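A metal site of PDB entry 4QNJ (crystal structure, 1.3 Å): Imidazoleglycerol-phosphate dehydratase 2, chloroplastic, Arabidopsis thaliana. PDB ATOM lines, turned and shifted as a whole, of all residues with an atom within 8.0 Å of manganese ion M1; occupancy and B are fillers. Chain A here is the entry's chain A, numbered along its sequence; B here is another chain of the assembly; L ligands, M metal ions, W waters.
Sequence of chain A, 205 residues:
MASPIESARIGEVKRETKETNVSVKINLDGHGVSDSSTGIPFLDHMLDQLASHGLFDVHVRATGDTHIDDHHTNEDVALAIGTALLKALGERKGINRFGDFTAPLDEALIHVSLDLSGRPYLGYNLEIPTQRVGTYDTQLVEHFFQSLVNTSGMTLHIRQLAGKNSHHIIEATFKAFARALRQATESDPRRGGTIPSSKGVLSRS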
ATOM      1  N   PHE A  42       9.468 -38.651  -1.819  1.00  0.00           N
ATOM      2  CA  PHE A  42       9.872 -37.749  -2.891  1.00  0.00           C
ATOM      3  C   PHE A  42       9.213 -38.156  -4.214  1.00  0.00           C
ATOM      4  O   PHE A  42       8.807 -37.305  -5.020  1.00  0.00           O
ATOM      5  CB  PHE A  42      11.391 -37.631  -3.047  1.00  0.00           C
ATOM      6  CG  PHE A  42      11.785 -36.448  -3.896  1.00  0.00           C
ATOM      7  CD1 PHE A  42      11.901 -35.200  -3.313  1.00  0.00           C
ATOM      8  CD2 PHE A  42      11.958 -36.562  -5.261  1.00  0.00           C
ATOM      9  CE1 PHE A  42      12.189 -34.091  -4.092  1.00  0.00           C
ATOM     10  CE2 PHE A  42      12.247 -35.453  -6.040  1.00  0.00           C
ATOM     11  CZ  PHE A  42      12.344 -34.215  -5.450  1.00  0.00           C
ATOM     12  N   HIS A  45       5.749 -36.937  -4.290  1.00  0.00           N
ATOM     13  CA  HIS A  45       5.747 -35.500  -4.635  1.00  0.00           C
ATOM     14  C   HIS A  45       5.847 -35.323  -6.170  1.00  0.00           C
ATOM     15  O   HIS A  45       5.148 -34.501  -6.751  1.00  0.00           O
ATOM     16  CB  HIS A  45       6.885 -34.786  -3.869  1.00  0.00           C
ATOM     17  CG  HIS A  45       6.987 -33.306  -4.123  1.00  0.00           C
ATOM     18  ND1 HIS A  45       5.891 -32.475  -4.242  1.00  0.00           N
ATOM     19  CD2 HIS A  45       8.074 -32.515  -4.280  1.00  0.00           C
ATOM     20  CE1 HIS A  45       6.304 -31.237  -4.452  1.00  0.00           C
ATOM     21  NE2 HIS A  45       7.621 -31.241  -4.477  1.00  0.00           N
ATOM     22  N   MET A  46       6.709 -36.109  -6.802  1.00  0.00           N
ATOM     23  CA  MET A  46       6.860 -36.032  -8.271  1.00  0.00           C
ATOM     24  C   MET A  46       5.606 -36.529  -9.017  1.00  0.00           C
ATOM     25  O   MET A  46       5.208 -35.957 -10.032  1.00  0.00           O
ATOM     26  CB  MET A  46       8.114 -36.776  -8.734  1.00  0.00           C
ATOM     27  CG  MET A  46       9.417 -36.120  -8.253  1.00  0.00           C
ATOM     28  SD  MET A  46       9.586 -34.374  -8.698  1.00  0.00           S
ATOM     29  CE  MET A  46       9.058 -33.571  -7.178  1.00  0.00           C
ATOM     30  N   GLN A  49       3.132 -33.873  -9.079  1.00  0.00           N
ATOM     31  CA  GLN A  49       3.498 -32.936 -10.158  1.00  0.00           C
ATOM     32  C   GLN A  49       2.994 -33.446 -11.518  1.00  0.00           C
ATOM     33  O   GLN A  49       2.478 -32.686 -12.339  1.00  0.00           O
ATOM     34  CB  GLN A  49       4.995 -32.689 -10.182  1.00  0.00           C
ATOM     35  CG  GLN A  49       5.437 -31.921  -8.952  1.00  0.00           C
ATOM     36  CD  GLN A  49       5.189 -30.453  -9.145  1.00  0.00           C
ATOM     37  OE1 GLN A  49       5.632 -29.879 -10.138  1.00  0.00           O
ATOM     38  NE2 GLN A  49       4.471 -29.847  -8.228  1.00  0.00           N
ATOM     39  N   LEU A 105      11.965 -24.289 -13.265  1.00  0.00           N
ATOM     40  CA  LEU A 105      11.654 -24.141 -11.846  1.00  0.00           C
ATOM     41  C   LEU A 105      12.818 -23.324 -11.319  1.00  0.00           C
ATOM     42  O   LEU A 105      13.919 -23.824 -11.146  1.00  0.00           O
ATOM     43  CB  LEU A 105      11.499 -25.469 -11.085  1.00  0.00           C
ATOM     44  CG  LEU A 105      10.797 -25.303  -9.705  1.00  0.00           C
ATOM     45  CD1 LEU A 105      10.662 -26.622  -8.965  1.00  0.00           C
ATOM     46  CD2 LEU A 105      11.374 -24.239  -8.792  1.00  0.00           C
ATOM     47  N   HIS A 167      16.476 -30.729  -6.186  1.00  0.00           N
ATOM     48  CA  HIS A 167      15.006 -30.776  -6.127  1.00  0.00           C
ATOM     49  C   HIS A 167      14.418 -29.980  -7.295  1.00  0.00           C
ATOM     50  O   HIS A 167      13.490 -30.443  -7.957  1.00  0.00           O
ATOM     51  CB  HIS A 167      14.583 -30.277  -4.746  1.00  0.00           C
ATOM     52  CG  HIS A 167      13.114 -30.334  -4.414  1.00  0.00           C
ATOM     53  ND1 HIS A 167      12.700 -30.639  -3.136  1.00  0.00           N
ATOM     54  CD2 HIS A 167      11.992 -29.985  -5.092  1.00  0.00           C
ATOM     55  CE1 HIS A 167      11.392 -30.489  -3.043  1.00  0.00           C
ATOM     56  NE2 HIS A 167      10.934 -30.113  -4.226  1.00  0.00           N
ATOM     57  N   HIS A 168      14.961 -28.804  -7.564  1.00  0.00           N
ATOM     58  CA  HIS A 168      14.481 -28.024  -8.719  1.00  0.00           C
ATOM     59  C   HIS A 168      14.664 -28.742 -10.060  1.00  0.00           C
ATOM     60  O   HIS A 168      13.779 -28.751 -10.902  1.00  0.00           O
ATOM     61  CB  HIS A 168      15.156 -26.664  -8.798  1.00  0.00           C
ATOM     62  CG  HIS A 168      14.750 -25.733  -7.704  1.00  0.00           C
ATOM     63  ND1 HIS A 168      15.339 -24.500  -7.539  1.00  0.00           N
ATOM     64  CD2 HIS A 168      13.837 -25.845  -6.704  1.00  0.00           C
ATOM     65  CE1 HIS A 168      14.780 -23.886  -6.507  1.00  0.00           C
ATOM     66  NE2 HIS A 168      13.870 -24.683  -5.990  1.00  0.00           N
ATOM     67  N   GLU A 171      12.157 -31.753 -10.150  1.00  0.00           N
ATOM     68  CA  GLU A 171      10.764 -31.279 -10.211  1.00  0.00           C
ATOM     69  C   GLU A 171      10.459 -30.617 -11.565  1.00  0.00           C
ATOM     70  O   GLU A 171       9.399 -30.866 -12.165  1.00  0.00           O
ATOM     71  CB  GLU A 171      10.460 -30.356  -9.035  1.00  0.00           C
ATOM     72  CG  GLU A 171       9.003 -29.945  -8.966  1.00  0.00           C
ATOM     73  CD  GLU A 171       8.632 -29.243  -7.683  1.00  0.00           C
ATOM     74  OE1 GLU A 171       9.219 -29.541  -6.633  1.00  0.00           O
ATOM     75  OE2 GLU A 171       7.744 -28.361  -7.752  1.00  0.00           O
ATOM     76  N   ALA A 172      11.397 -29.799 -12.061  1.00  0.00           N
ATOM     77  CA  ALA A 172      11.220 -29.199 -13.402  1.00  0.00           C
ATOM     78  C   ALA A 172      11.108 -30.286 -14.483  1.00  0.00           C
ATOM     79  O   ALA A 172      10.326 -30.147 -15.440  1.00  0.00           O
ATOM     80  CB  ALA A 172      12.348 -28.224 -13.720  1.00  0.00           C
ATOM     81  N   LYS A 175       7.583 -31.541 -14.338  1.00  0.00           N
ATOM     82  CA  LYS A 175       6.674 -30.538 -14.917  1.00  0.00           C
ATOM     83  C   LYS A 175       6.706 -30.589 -16.439  1.00  0.00           C
ATOM     84  O   LYS A 175       5.659 -30.570 -17.106  1.00  0.00           O
ATOM     85  CB  LYS A 175       7.010 -29.115 -14.485  1.00  0.00           C
ATOM     86  CG  LYS A 175       6.882 -28.834 -13.007  1.00  0.00           C
ATOM     87  CD  LYS A 175       7.169 -27.365 -12.749  1.00  0.00           C
ATOM     88  CE  LYS A 175       7.648 -27.074 -11.343  1.00  0.00           C
ATOM     89  NZ  LYS A 175       6.607 -27.493 -10.376  1.00  0.00           N
ATOM     90  N   GLU B  19       1.972 -27.127   1.587  1.00  0.00           N
ATOM     91  CA  GLU B  19       3.238 -27.788   2.016  1.00  0.00           C
ATOM     92  C   GLU B  19       3.709 -27.442   3.435  1.00  0.00           C
ATOM     93  O   GLU B  19       4.347 -28.261   4.103  1.00  0.00           O
ATOM     94  CB  GLU B  19       4.383 -27.459   1.055  1.00  0.00           C
ATOM     95  CG  GLU B  19       4.191 -27.978  -0.353  1.00  0.00           C
ATOM     96  CD  GLU B  19       3.650 -26.926  -1.297  1.00  0.00           C
ATOM     97  OE1 GLU B  19       3.709 -25.724  -0.978  1.00  0.00           O
ATOM     98  OE2 GLU B  19       3.159 -27.305  -2.371  1.00  0.00           O
ATOM     99  N   ASP B  65       6.258 -30.410   5.266  1.00  0.00           N
ATOM    100  CA  ASP B  65       6.463 -31.709   4.641  1.00  0.00           C
ATOM    101  C   ASP B  65       7.927 -32.202   4.618  1.00  0.00           C
ATOM    102  O   ASP B  65       8.458 -32.589   3.563  1.00  0.00           O
ATOM    103  CB  ASP B  65       5.818 -31.754   3.248  1.00  0.00           C
ATOM    104  CG  ASP B  65       6.371 -30.706   2.294  1.00  0.00           C
ATOM    105  OD1 ASP B  65       7.303 -29.951   2.656  1.00  0.00           O
ATOM    106  OD2 ASP B  65       5.834 -30.626   1.174  1.00  0.00           O
ATOM    107  N   ILE B  68       9.267 -35.332   2.791  1.00  0.00           N
ATOM    108  CA  ILE B  68       9.643 -35.218   1.368  1.00  0.00           C
ATOM    109  C   ILE B  68      11.094 -34.770   1.237  1.00  0.00           C
ATOM    110  O   ILE B  68      11.899 -35.378   0.536  1.00  0.00           O
ATOM    111  CB  ILE B  68       8.702 -34.264   0.620  1.00  0.00           C
ATOM    112  CG1 ILE B  68       7.314 -34.906   0.572  1.00  0.00           C
ATOM    113  CG2 ILE B  68       9.245 -33.963  -0.782  1.00  0.00           C
ATOM    114  CD1 ILE B  68       6.259 -34.002  -0.002  1.00  0.00           C
ATOM    115  N   ASP B  69      11.367 -33.632   1.870  1.00  0.00           N
ATOM    116  CA  ASP B  69      12.726 -33.131   2.210  1.00  0.00           C
ATOM    117  C   ASP B  69      12.555 -31.780   2.890  1.00  0.00           C
ATOM    118  O   ASP B  69      11.416 -31.327   3.113  1.00  0.00           O
ATOM    119  CB  ASP B  69      13.733 -33.073   1.061  1.00  0.00           C
ATOM    120  CG  ASP B  69      13.421 -32.014   0.038  1.00  0.00           C
ATOM    121  OD1 ASP B  69      12.382 -31.370   0.205  1.00  0.00           O
ATOM    122  OD2 ASP B  69      14.247 -31.828  -0.914  1.00  0.00           O
ATOM    123  N   HIS B  71      13.316 -28.959   1.906  1.00  0.00           N
ATOM    124  CA  HIS B  71      13.292 -27.860   0.935  1.00  0.00           C
ATOM    125  C   HIS B  71      12.111 -26.899   1.107  1.00  0.00           C
ATOM    126  O   HIS B  71      12.296 -25.677   1.178  1.00  0.00           O
ATOM    127  CB  HIS B  71      13.254 -28.428  -0.474  1.00  0.00           C
ATOM    128  CG  HIS B  71      13.423 -27.412  -1.568  1.00  0.00           C
ATOM    129  ND1 HIS B  71      14.438 -27.510  -2.497  1.00  0.00           N
ATOM    130  CD2 HIS B  71      12.702 -26.316  -1.926  1.00  0.00           C
ATOM    131  CE1 HIS B  71      14.348 -26.525  -3.361  1.00  0.00           C
ATOM    132  NE2 HIS B  71      13.306 -25.785  -3.042  1.00  0.00           N
ATOM    133  N   HIS B  72      10.893 -27.427   1.126  1.00  0.00           N
ATOM    134  CA  HIS B  72       9.725 -26.522   1.142  1.00  0.00           C
ATOM    135  C   HIS B  72       9.675 -25.695   2.440  1.00  0.00           C
ATOM    136  O   HIS B  72       9.398 -24.498   2.412  1.00  0.00           O
ATOM    137  CB  HIS B  72       8.399 -27.273   0.935  1.00  0.00           C
ATOM    138  CG  HIS B  72       8.288 -28.040  -0.349  1.00  0.00           C
ATOM    139  ND1 HIS B  72       7.458 -29.137  -0.461  1.00  0.00           N
ATOM    140  CD2 HIS B  72       8.882 -27.912  -1.568  1.00  0.00           C
ATOM    141  CE1 HIS B  72       7.527 -29.644  -1.681  1.00  0.00           C
ATOM    142  NE2 HIS B  72       8.386 -28.908  -2.374  1.00  0.00           N
ATOM    143  N   GLU B  75      12.470 -23.002   2.359  1.00  0.00           N
ATOM    144  CA  GLU B  75      12.080 -21.927   1.427  1.00  0.00           C
ATOM    145  C   GLU B  75      10.990 -21.036   2.025  1.00  0.00           C
ATOM    146  O   GLU B  75      11.079 -19.803   2.020  1.00  0.00           O
ATOM    147  CB  GLU B  75      11.628 -22.540   0.106  1.00  0.00           C
ATOM    148  CG  GLU B  75      11.095 -21.514  -0.884  1.00  0.00           C
ATOM    149  CD  GLU B  75      10.983 -22.014  -2.322  1.00  0.00           C
ATOM    150  OE1 GLU B  75      11.259 -23.212  -2.559  1.00  0.00           O
ATOM    151  OE2 GLU B  75      10.628 -21.190  -3.192  1.00  0.00           O
HETATM  152  C1  LIG L   1      10.660 -26.668  -4.639  1.00  0.00           C
HETATM  153  O1  LIG L   1       9.532 -27.163  -4.737  1.00  0.00           O
HETATM  154  O2  LIG L   1      10.827 -25.380  -4.793  1.00  0.00           O
HETATM  155 MN    MN M   1       8.827 -29.269  -4.571  1.00  0.00          MN
HETATM  156 MN    MN M   2      12.507 -24.051  -4.264  1.00  0.00          MN
HETATM  157  O   HOH W   1       6.864 -28.270  -5.193  1.00  0.00           O
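Of the 17 residues printed, 4 come within 4 Å of manganese ion M1.
The nearest printed residue that does not touch manganese ion M1 is Met 46 (5.0 Å).
OE1 of Glu 171 binds manganese ion M1 (2.1 Å).
Manganese ion M1 is bound by O1 of the ligand (2.2 Å).
A ring nitrogen (NE2) of His 72 of chain B is bound to manganese ion M1 (2.3 Å).
Water W1 is bound to manganese ion M1 (2.3 Å).
Manganese ion M1 is bound by NE2 of His 167 (2.3 Å).
A ring nitrogen (NE2) of His 45 is bound to manganese ion M1.
Manganese ion M1 has six donor atoms within binding distance.
The side-chain carboxylate of Glu 171 lies within salt-bridge range of the side-chain amino group of Lys 175 (3.0 Å).
A ring nitrogen (ND1) of His 72 of chain B lies within hydrogen-bond range of the side-chain carboxylate (OD2) of Asp 65 of chain B (2.7 Å).
The side-chain carboxylate (OD2) of Asp 69 of chain B sits at hydrogen-bond distance from a ring nitrogen (ND1) of His 167, 3.0 Å away.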
